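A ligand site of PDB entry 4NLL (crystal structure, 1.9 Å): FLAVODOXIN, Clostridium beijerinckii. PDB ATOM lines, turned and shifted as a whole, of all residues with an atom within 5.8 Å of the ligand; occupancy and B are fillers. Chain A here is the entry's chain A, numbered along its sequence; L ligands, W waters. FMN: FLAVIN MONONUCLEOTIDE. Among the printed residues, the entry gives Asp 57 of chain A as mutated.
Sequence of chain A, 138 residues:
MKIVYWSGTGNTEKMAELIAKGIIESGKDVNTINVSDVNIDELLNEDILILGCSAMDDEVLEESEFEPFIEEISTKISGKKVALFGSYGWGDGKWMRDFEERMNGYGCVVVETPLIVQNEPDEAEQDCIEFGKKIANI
The backbone NH (N) of Thr 9 lies within hydrogen-bond range of an oxygen (O3P) of the ligand (2.8 Å). The side-chain hydroxyl (OG1) of Thr 9 lies within hydrogen-bond range of an oxygen (O3P) of the ligand, 2.6 Å away. An oxygen (O3P) of the ligand sits at hydrogen-bond distance from the backbone NH (N) of Asn 11 (3.0 Å). The side-chain amide oxygen (OD1) of Asn 11 sits at hydrogen-bond distance from an oxygen (O4') of the ligand, at 2.7 Å. N of Ala 55 lies within hydrogen-bond range of O2' of the ligand, at 3.4 Å. The backbone carbonyl oxygen (O) of Ala 55 lies within hydrogen-bond range of an oxygen (O2') of the ligand (2.7 Å). N of Thr 12 lies within hydrogen-bond range of O2P of the ligand, 2.7 Å away. O2P of the ligand lies within hydrogen-bond range of OG1 of Thr 12. The backbone NH (N) of Gly 91 lies within hydrogen-bond range of an oxygen (O2) of the ligand (2.7 Å). OG of Ser 7 sits at hydrogen-bond distance from O2P of the ligand, at 2.7 Å. N of Gly 8 sits at hydrogen-bond distance from O1P of the ligand. O1P of the ligand is in hydrogen-bond range of OG of Ser 54 (2.8 Å). O4' of the ligand lies within hydrogen-bond range of OG of Ser 87 (2.9 Å). N of Glu 59 lies within hydrogen-bond range of O4 of the ligand (3.0 Å). A nitrogen (N3) of the ligand sits at hydrogen-bond distance from the side-chain carboxylate of Glu 59. An oxygen (O3P) of the ligand lies within hydrogen-bond range of the backbone NH of Gly 10, at 3.0 Å. The backbone NH (N) of Gly 89 is in hydrogen-bond range of an oxygen (O2) of the ligand (3.0 Å). N of Trp 90 lies within hydrogen-bond range of O2 of the ligand. The backbone NH of Asp 57 is in hydrogen-bond range of a nitrogen (N5) of the ligand, at 3.4 Å.
The backbone carbonyl oxygen of Ser 87 sits at hydrogen-bond distance from the backbone NH of Ala 55 (3.2 Å). The backbone NH of Ser 87 is in hydrogen-bond range of the side-chain hydroxyl of Thr 12 (3.4 Å). N of Gly 10 lies within hydrogen-bond range of OG of Ser 7, 3.0 Å away. O of Asn 119 lies within hydrogen-bond range of OG of Ser 87 (2.7 Å). The side-chain hydroxyl (OG) of Ser 87 lies close to the backbone carbonyl oxygen (O) of Val 117. The side-chain carboxylate (OE1) of Glu 59 is in hydrogen-bond range of the backbone NH (N) of Trp 95, at 3.1 Å. N of Asn 119 lies within hydrogen-bond range of O of Tyr 88 (2.8 Å). The backbone NH of Tyr 88 lies within hydrogen-bond range of the backbone carbonyl oxygen of Val 117, at 3.0 Å.
Water W4 lies within hydrogen-bond range of an oxygen (O3') of the ligand (2.6 Å), the side-chain amide oxygen of Asn 119 (2.8 Å) and the side-chain amide oxygen of Asn 11 (3.3 Å). Water W1 lies within hydrogen-bond range of OE1 of Glu 59, O2 of the ligand and N of Asp 92.
The backbone carbonyl oxygen of Met 56 lies close to an oxygen (O4) of the ligand (3.4 Å). Trp 6 touches the ligand. Asp 58 touches the ligand (OD1 to O4, 3.6 Å). Tyr 88 touches the ligand. Asn 119 touches the ligand (CA to O4', 3.6 Å). Hydrophobic or aromatic side chains that line the ligand: Trp 6, Ala 55, Met 56, Tyr 88 and Trp 90. The nearest printed residue that does not touch the ligand is Glu 13 (4.5 Å).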
ATOM      1  N   TRP A   6      -7.258   8.942 -18.690  1.00  0.00           N
ATOM      2  CA  TRP A   6      -7.887   7.630 -18.706  1.00  0.00           C
ATOM      3  C   TRP A   6      -7.300   6.930 -17.477  1.00  0.00           C
ATOM      4  O   TRP A   6      -6.093   7.076 -17.187  1.00  0.00           O
ATOM      5  CB  TRP A   6      -7.530   6.819 -19.970  1.00  0.00           C
ATOM      6  CG  TRP A   6      -8.247   5.463 -19.987  1.00  0.00           C
ATOM      7  CD1 TRP A   6      -9.491   5.213 -20.492  1.00  0.00           C
ATOM      8  CD2 TRP A   6      -7.793   4.227 -19.412  1.00  0.00           C
ATOM      9  NE1 TRP A   6      -9.851   3.915 -20.251  1.00  0.00           N
ATOM     10  CE2 TRP A   6      -8.832   3.280 -19.593  1.00  0.00           C
ATOM     11  CE3 TRP A   6      -6.615   3.826 -18.744  1.00  0.00           C
ATOM     12  CZ2 TRP A   6      -8.732   1.946 -19.130  1.00  0.00           C
ATOM     13  CZ3 TRP A   6      -6.520   2.499 -18.285  1.00  0.00           C
ATOM     14  CH2 TRP A   6      -7.578   1.583 -18.481  1.00  0.00           C
ATOM     15  N   SER A   7      -8.137   6.221 -16.733  1.00  0.00           N
ATOM     16  CA  SER A   7      -7.670   5.496 -15.557  1.00  0.00           C
ATOM     17  C   SER A   7      -8.448   4.198 -15.404  1.00  0.00           C
ATOM     18  O   SER A   7      -9.687   4.214 -15.404  1.00  0.00           O
ATOM     19  CB  SER A   7      -7.825   6.380 -14.324  1.00  0.00           C
ATOM     20  OG  SER A   7      -7.263   5.763 -13.178  1.00  0.00           O
ATOM     21  N   GLY A   8      -7.743   3.085 -15.264  1.00  0.00           N
ATOM     22  CA  GLY A   8      -8.394   1.789 -15.141  1.00  0.00           C
ATOM     23  C   GLY A   8      -8.768   1.354 -13.734  1.00  0.00           C
ATOM     24  O   GLY A   8      -9.695   0.550 -13.560  1.00  0.00           O
ATOM     25  N   THR A   9      -8.025   1.807 -12.728  1.00  0.00           N
ATOM     26  CA  THR A   9      -8.320   1.450 -11.340  1.00  0.00           C
ATOM     27  C   THR A   9      -8.364   2.702 -10.461  1.00  0.00           C
ATOM     28  O   THR A   9      -8.570   2.600  -9.242  1.00  0.00           O
ATOM     29  CB  THR A   9      -7.282   0.446 -10.752  1.00  0.00           C
ATOM     30  OG1 THR A   9      -6.057   1.122 -10.453  1.00  0.00           O
ATOM     31  CG2 THR A   9      -7.023  -0.692 -11.726  1.00  0.00           C
ATOM     32  N   GLY A  10      -8.113   3.863 -11.049  1.00  0.00           N
ATOM     33  CA  GLY A  10      -8.177   5.106 -10.293  1.00  0.00           C
ATOM     34  C   GLY A  10      -6.865   5.770  -9.945  1.00  0.00           C
ATOM     35  O   GLY A  10      -6.880   6.850  -9.374  1.00  0.00           O
ATOM     36  N   ASN A  11      -5.725   5.175 -10.291  1.00  0.00           N
ATOM     37  CA  ASN A  11      -4.445   5.788  -9.928  1.00  0.00           C
ATOM     38  C   ASN A  11      -4.195   7.086 -10.650  1.00  0.00           C
ATOM     39  O   ASN A  11      -3.880   8.104 -10.029  1.00  0.00           O
ATOM     40  CB  ASN A  11      -3.283   4.806 -10.129  1.00  0.00           C
ATOM     41  CG  ASN A  11      -3.372   3.625  -9.191  1.00  0.00           C
ATOM     42  OD1 ASN A  11      -2.801   2.572  -9.433  1.00  0.00           O
ATOM     43  ND2 ASN A  11      -4.105   3.804  -8.082  1.00  0.00           N
ATOM     44  N   THR A  12      -4.339   7.058 -11.974  1.00  0.00           N
ATOM     45  CA  THR A  12      -4.152   8.257 -12.788  1.00  0.00           C
ATOM     46  C   THR A  12      -5.266   9.271 -12.509  1.00  0.00           C
ATOM     47  O   THR A  12      -5.020  10.486 -12.540  1.00  0.00           O
ATOM     48  CB  THR A  12      -4.131   7.904 -14.280  1.00  0.00           C
ATOM     49  OG1 THR A  12      -3.105   6.937 -14.509  1.00  0.00           O
ATOM     50  CG2 THR A  12      -3.848   9.146 -15.131  1.00  0.00           C
ATOM     51  N   GLU A  13      -6.469   8.798 -12.220  1.00  0.00           N
ATOM     52  CA  GLU A  13      -7.579   9.688 -11.911  1.00  0.00           C
ATOM     53  C   GLU A  13      -7.217  10.510 -10.658  1.00  0.00           C
ATOM     54  O   GLU A  13      -7.419  11.720 -10.621  1.00  0.00           O
ATOM     55  CB  GLU A  13      -8.856   8.906 -11.662  1.00  0.00           C
ATOM     56  CG  GLU A  13     -10.052   9.781 -11.325  1.00  0.00           C
ATOM     57  CD  GLU A  13     -11.365   9.028 -11.230  1.00  0.00           C
ATOM     58  OE1 GLU A  13     -11.439   7.852 -11.649  1.00  0.00           O
ATOM     59  OE2 GLU A  13     -12.337   9.630 -10.721  1.00  0.00           O
ATOM     60  N   SER A  54      -2.323   5.751 -17.822  1.00  0.00           N
ATOM     61  CA  SER A  54      -1.460   4.737 -17.214  1.00  0.00           C
ATOM     62  C   SER A  54      -0.811   3.855 -18.268  1.00  0.00           C
ATOM     63  O   SER A  54      -1.232   3.841 -19.443  1.00  0.00           O
ATOM     64  CB  SER A  54      -2.273   3.869 -16.254  1.00  0.00           C
ATOM     65  OG  SER A  54      -3.452   3.412 -16.895  1.00  0.00           O
ATOM     66  N   ALA A  55       0.218   3.126 -17.841  1.00  0.00           N
ATOM     67  CA  ALA A  55       0.961   2.251 -18.740  1.00  0.00           C
ATOM     68  C   ALA A  55       0.195   0.934 -18.952  1.00  0.00           C
ATOM     69  O   ALA A  55      -0.139   0.254 -17.988  1.00  0.00           O
ATOM     70  CB  ALA A  55       2.348   1.965 -18.156  1.00  0.00           C
ATOM     71  N   MET A  56      -0.126   0.640 -20.200  1.00  0.00           N
ATOM     72  CA  MET A  56      -0.801  -0.619 -20.541  1.00  0.00           C
ATOM     73  C   MET A  56       0.218  -1.473 -21.285  1.00  0.00           C
ATOM     74  O   MET A  56       1.322  -1.011 -21.571  1.00  0.00           O
ATOM     75  CB  MET A  56      -2.065  -0.379 -21.376  1.00  0.00           C
ATOM     76  CG  MET A  56      -3.216   0.232 -20.593  1.00  0.00           C
ATOM     77  SD  MET A  56      -3.831  -0.773 -19.179  1.00  0.00           S
ATOM     78  CE  MET A  56      -3.500   0.354 -17.812  1.00  0.00           C
ATOM     79  N   ASP A  57      -0.109  -2.720 -21.603  1.00  0.00           N
ATOM     80  CA  ASP A  57       0.913  -3.548 -22.220  1.00  0.00           C
ATOM     81  C   ASP A  57       1.031  -3.543 -23.731  1.00  0.00           C
ATOM     82  O   ASP A  57       0.047  -3.473 -24.461  1.00  0.00           O
ATOM     83  CB  ASP A  57       0.901  -4.976 -21.648  1.00  0.00           C
ATOM     84  CG  ASP A  57      -0.131  -5.864 -22.314  1.00  0.00           C
ATOM     85  OD1 ASP A  57      -1.332  -5.509 -22.321  1.00  0.00           O
ATOM     86  OD2 ASP A  57       0.274  -6.942 -22.804  1.00  0.00           O
ATOM     87  N   ASP A  58       2.277  -3.520 -24.179  1.00  0.00           N
ATOM     88  CA  ASP A  58       3.400  -3.471 -23.255  1.00  0.00           C
ATOM     89  C   ASP A  58       4.096  -2.130 -23.345  1.00  0.00           C
ATOM     90  O   ASP A  58       4.777  -1.838 -24.319  1.00  0.00           O
ATOM     91  CB  ASP A  58       4.389  -4.589 -23.536  1.00  0.00           C
ATOM     92  CG  ASP A  58       5.288  -4.819 -22.373  1.00  0.00           C
ATOM     93  OD1 ASP A  58       4.759  -5.260 -21.325  1.00  0.00           O
ATOM     94  OD2 ASP A  58       6.490  -4.515 -22.483  1.00  0.00           O
ATOM     95  N   GLU A  59       3.934  -1.329 -22.298  1.00  0.00           N
ATOM     96  CA  GLU A  59       4.493   0.018 -22.252  1.00  0.00           C
ATOM     97  C   GLU A  59       3.899   0.851 -23.385  1.00  0.00           C
ATOM     98  O   GLU A  59       4.607   1.553 -24.108  1.00  0.00           O
ATOM     99  CB  GLU A  59       6.027  -0.003 -22.327  1.00  0.00           C
ATOM    100  CG  GLU A  59       6.718  -0.681 -21.134  1.00  0.00           C
ATOM    101  CD  GLU A  59       6.496   0.016 -19.780  1.00  0.00           C
ATOM    102  OE1 GLU A  59       6.122   1.203 -19.727  1.00  0.00           O
ATOM    103  OE2 GLU A  59       6.731  -0.636 -18.756  1.00  0.00           O
ATOM    104  N   VAL A  60       2.573   0.789 -23.509  1.00  0.00           N
ATOM    105  CA  VAL A  60       1.836   1.546 -24.536  1.00  0.00           C
ATOM    106  C   VAL A  60       0.682   2.289 -23.872  1.00  0.00           C
ATOM    107  O   VAL A  60       0.349   2.030 -22.705  1.00  0.00           O
ATOM    108  CB  VAL A  60       1.232   0.618 -25.645  1.00  0.00           C
ATOM    109  CG1 VAL A  60       2.325  -0.128 -26.366  1.00  0.00           C
ATOM    110  CG2 VAL A  60       0.216  -0.356 -25.054  1.00  0.00           C
ATOM    111  N   SER A  87       0.318   7.005 -14.191  1.00  0.00           N
ATOM    112  CA  SER A  87       0.753   6.056 -13.168  1.00  0.00           C
ATOM    113  C   SER A  87       1.204   4.812 -13.900  1.00  0.00           C
ATOM    114  O   SER A  87       0.717   4.508 -15.009  1.00  0.00           O
ATOM    115  CB  SER A  87      -0.402   5.752 -12.212  1.00  0.00           C
ATOM    116  OG  SER A  87      -0.050   4.777 -11.238  1.00  0.00           O
ATOM    117  N   TYR A  88       2.161   4.084 -13.326  1.00  0.00           N
ATOM    118  CA  TYR A  88       2.650   2.860 -13.935  1.00  0.00           C
ATOM    119  C   TYR A  88       2.900   1.844 -12.839  1.00  0.00           C
ATOM    120  O   TYR A  88       2.822   2.174 -11.659  1.00  0.00           O
ATOM    121  CB  TYR A  88       3.922   3.110 -14.762  1.00  0.00           C
ATOM    122  CG  TYR A  88       5.121   3.550 -13.946  1.00  0.00           C
ATOM    123  CD1 TYR A  88       5.208   4.853 -13.442  1.00  0.00           C
ATOM    124  CD2 TYR A  88       6.155   2.658 -13.645  1.00  0.00           C
ATOM    125  CE1 TYR A  88       6.294   5.246 -12.655  1.00  0.00           C
ATOM    126  CE2 TYR A  88       7.230   3.043 -12.863  1.00  0.00           C
ATOM    127  CZ  TYR A  88       7.288   4.325 -12.364  1.00  0.00           C
ATOM    128  OH  TYR A  88       8.340   4.680 -11.558  1.00  0.00           O
ATOM    129  N   GLY A  89       3.195   0.611 -13.220  1.00  0.00           N
ATOM    130  CA  GLY A  89       3.378  -0.423 -12.230  1.00  0.00           C
ATOM    131  C   GLY A  89       4.787  -0.942 -12.118  1.00  0.00           C
ATOM    132  O   GLY A  89       5.582  -0.434 -11.352  1.00  0.00           O
ATOM    133  N   TRP A  90       5.120  -1.907 -12.965  1.00  0.00           N
ATOM    134  CA  TRP A  90       6.415  -2.563 -12.909  1.00  0.00           C
ATOM    135  C   TRP A  90       7.499  -2.047 -13.862  1.00  0.00           C
ATOM    136  O   TRP A  90       8.651  -2.462 -13.758  1.00  0.00           O
ATOM    137  CB  TRP A  90       6.216  -4.056 -13.110  1.00  0.00           C
ATOM    138  CG  TRP A  90       5.504  -4.384 -14.395  1.00  0.00           C
ATOM    139  CD1 TRP A  90       6.064  -4.515 -15.629  1.00  0.00           C
ATOM    140  CD2 TRP A  90       4.093  -4.636 -14.560  1.00  0.00           C
ATOM    141  NE1 TRP A  90       5.088  -4.819 -16.557  1.00  0.00           N
ATOM    142  CE2 TRP A  90       3.883  -4.904 -15.922  1.00  0.00           C
ATOM    143  CE3 TRP A  90       2.997  -4.647 -13.683  1.00  0.00           C
ATOM    144  CZ2 TRP A  90       2.612  -5.193 -16.444  1.00  0.00           C
ATOM    145  CZ3 TRP A  90       1.735  -4.928 -14.201  1.00  0.00           C
ATOM    146  CH2 TRP A  90       1.557  -5.193 -15.571  1.00  0.00           C
ATOM    147  N   GLY A  91       7.136  -1.173 -14.794  1.00  0.00           N
ATOM    148  CA  GLY A  91       8.129  -0.706 -15.757  1.00  0.00           C
ATOM    149  C   GLY A  91       9.006   0.414 -15.228  1.00  0.00           C
ATOM    150  O   GLY A  91       9.045   0.669 -14.037  1.00  0.00           O
ATOM    151  N   ASP A  92       9.719   1.070 -16.128  1.00  0.00           N
ATOM    152  CA  ASP A  92      10.574   2.177 -15.755  1.00  0.00           C
ATOM    153  C   ASP A  92      10.204   3.468 -16.480  1.00  0.00           C
ATOM    154  O   ASP A  92      11.049   4.359 -16.631  1.00  0.00           O
ATOM    155  CB  ASP A  92      12.071   1.843 -15.948  1.00  0.00           C
ATOM    156  CG  ASP A  92      12.457   1.600 -17.422  1.00  0.00           C
ATOM    157  OD1 ASP A  92      11.826   2.137 -18.357  1.00  0.00           O
ATOM    158  OD2 ASP A  92      13.447   0.863 -17.632  1.00  0.00           O
ATOM    159  N   TRP A  95       6.657   3.734 -21.476  1.00  0.00           N
ATOM    160  CA  TRP A  95       5.450   4.230 -22.150  1.00  0.00           C
ATOM    161  C   TRP A  95       5.392   5.765 -22.159  1.00  0.00           C
ATOM    162  O   TRP A  95       4.909   6.363 -23.130  1.00  0.00           O
ATOM    163  CB  TRP A  95       4.169   3.624 -21.541  1.00  0.00           C
ATOM    164  CG  TRP A  95       3.346   4.525 -20.616  1.00  0.00           C
ATOM    165  CD1 TRP A  95       2.121   5.065 -20.892  1.00  0.00           C
ATOM    166  CD2 TRP A  95       3.692   4.961 -19.295  1.00  0.00           C
ATOM    167  NE1 TRP A  95       1.683   5.817 -19.826  1.00  0.00           N
ATOM    168  CE2 TRP A  95       2.627   5.777 -18.829  1.00  0.00           C
ATOM    169  CE3 TRP A  95       4.795   4.751 -18.455  1.00  0.00           C
ATOM    170  CZ2 TRP A  95       2.639   6.374 -17.560  1.00  0.00           C
ATOM    171  CZ3 TRP A  95       4.806   5.348 -17.185  1.00  0.00           C
ATOM    172  CH2 TRP A  95       3.729   6.151 -16.757  1.00  0.00           C
ATOM    173  N   VAL A 117       4.193   8.333 -11.641  1.00  0.00           N
ATOM    174  CA  VAL A 117       4.151   7.844 -10.273  1.00  0.00           C
ATOM    175  C   VAL A 117       3.813   6.376 -10.327  1.00  0.00           C
ATOM    176  O   VAL A 117       3.027   5.946 -11.181  1.00  0.00           O
ATOM    177  CB  VAL A 117       3.034   8.559  -9.455  1.00  0.00           C
ATOM    178  CG1 VAL A 117       2.814   7.869  -8.112  1.00  0.00           C
ATOM    179  CG2 VAL A 117       3.403  10.025  -9.238  1.00  0.00           C
ATOM    180  N   GLN A 118       4.439   5.605  -9.447  1.00  0.00           N
ATOM    181  CA  GLN A 118       4.189   4.171  -9.385  1.00  0.00           C
ATOM    182  C   GLN A 118       2.950   3.910  -8.547  1.00  0.00           C
ATOM    183  O   GLN A 118       2.860   4.361  -7.391  1.00  0.00           O
ATOM    184  CB  GLN A 118       5.392   3.441  -8.791  1.00  0.00           C
ATOM    185  CG  GLN A 118       5.338   1.936  -8.969  1.00  0.00           C
ATOM    186  CD  GLN A 118       6.622   1.232  -8.555  1.00  0.00           C
ATOM    187  OE1 GLN A 118       7.580   1.858  -8.092  1.00  0.00           O
ATOM    188  NE2 GLN A 118       6.643  -0.091  -8.720  1.00  0.00           N
ATOM    189  N   ASN A 119       2.000   3.199  -9.138  1.00  0.00           N
ATOM    190  CA  ASN A 119       0.744   2.826  -8.478  1.00  0.00           C
ATOM    191  C   ASN A 119      -0.003   4.059  -7.937  1.00  0.00           C
ATOM    192  O   ASN A 119       0.020   5.096  -8.588  1.00  0.00           O
ATOM    193  CB  ASN A 119       1.021   1.759  -7.416  1.00  0.00           C
ATOM    194  CG  ASN A 119       1.800   0.578  -7.997  1.00  0.00           C
ATOM    195  OD1 ASN A 119       1.352  -0.090  -8.932  1.00  0.00           O
ATOM    196  ND2 ASN A 119       2.999   0.356  -7.484  1.00  0.00           N
ATOM    197  N   GLU A 120      -0.671   3.959  -6.798  1.00  0.00           N
ATOM    198  CA  GLU A 120      -1.422   5.115  -6.304  1.00  0.00           C
ATOM    199  C   GLU A 120      -0.502   6.208  -5.780  1.00  0.00           C
ATOM    200  O   GLU A 120       0.518   5.915  -5.158  1.00  0.00           O
ATOM    201  CB  GLU A 120      -2.423   4.708  -5.209  1.00  0.00           C
ATOM    202  CG  GLU A 120      -3.452   5.796  -4.912  1.00  0.00           C
ATOM    203  CD  GLU A 120      -4.557   5.372  -3.951  1.00  0.00           C
ATOM    204  OE1 GLU A 120      -5.390   4.514  -4.343  1.00  0.00           O
ATOM    205  OE2 GLU A 120      -4.616   5.917  -2.826  1.00  0.00           O
HETATM  206  N1  FMN L   1       2.668  -1.091 -15.758  1.00  0.00           N
HETATM  207  C2  FMN L   1       3.873  -0.875 -16.307  1.00  0.00           C
HETATM  208  O2  FMN L   1       4.729  -0.292 -15.674  1.00  0.00           O
HETATM  209  N3  FMN L   1       4.120  -1.319 -17.622  1.00  0.00           N
HETATM  210  C4  FMN L   1       3.267  -2.045 -18.394  1.00  0.00           C
HETATM  211  O4  FMN L   1       3.575  -2.424 -19.499  1.00  0.00           O
HETATM  212  C4A FMN L   1       1.951  -2.306 -17.768  1.00  0.00           C
HETATM  213  N5  FMN L   1       1.049  -3.025 -18.413  1.00  0.00           N
HETATM  214  C5A FMN L   1      -0.176  -3.237 -17.802  1.00  0.00           C
HETATM  215  C6  FMN L   1      -1.159  -4.001 -18.484  1.00  0.00           C
HETATM  216  C7  FMN L   1      -2.421  -4.162 -17.957  1.00  0.00           C
HETATM  217  C7M FMN L   1      -3.427  -5.039 -18.659  1.00  0.00           C
HETATM  218  C8  FMN L   1      -2.755  -3.528 -16.719  1.00  0.00           C
HETATM  219  C8M FMN L   1      -4.133  -3.640 -16.125  1.00  0.00           C
HETATM  220  C9  FMN L   1      -1.809  -2.813 -16.009  1.00  0.00           C
HETATM  221  C9A FMN L   1      -0.505  -2.636 -16.531  1.00  0.00           C
HETATM  222  N10 FMN L   1       0.492  -1.943 -15.855  1.00  0.00           N
HETATM  223  C10 FMN L   1       1.740  -1.753 -16.409  1.00  0.00           C
HETATM  224  C1' FMN L   1       0.226  -1.469 -14.506  1.00  0.00           C
HETATM  225  C2' FMN L   1      -0.552  -0.152 -14.506  1.00  0.00           C
HETATM  226  O2' FMN L   1       0.077   0.810 -15.353  1.00  0.00           O
HETATM  227  C3' FMN L   1      -0.600   0.394 -13.083  1.00  0.00           C
HETATM  228  O3' FMN L   1      -1.248  -0.556 -12.239  1.00  0.00           O
HETATM  229  C4' FMN L   1      -1.210   1.783 -12.865  1.00  0.00           C
HETATM  230  O4' FMN L   1      -1.119   2.120 -11.472  1.00  0.00           O
HETATM  231  C5' FMN L   1      -2.672   1.792 -13.293  1.00  0.00           C
HETATM  232  O5' FMN L   1      -3.191   3.099 -13.151  1.00  0.00           O
HETATM  233  P   FMN L   1      -4.686   3.432 -13.476  1.00  0.00           P
HETATM  234  O1P FMN L   1      -5.052   2.664 -14.667  1.00  0.00           O
HETATM  235  O2P FMN L   1      -4.716   4.898 -13.556  1.00  0.00           O
HETATM  236  O3P FMN L   1      -5.531   2.976 -12.264  1.00  0.00           O
HETATM  237  O   HOH W   1       6.573   1.999 -17.139  1.00  0.00           O
HETATM  238  O   HOH W   2      -3.706  -1.462 -13.276  1.00  0.00           O
HETATM  239  O   HOH W   3      -5.466  -0.083 -14.880  1.00  0.00           O
HETATM  240  O   HOH W   4      -1.314  -0.332  -9.632  1.00  0.00           O
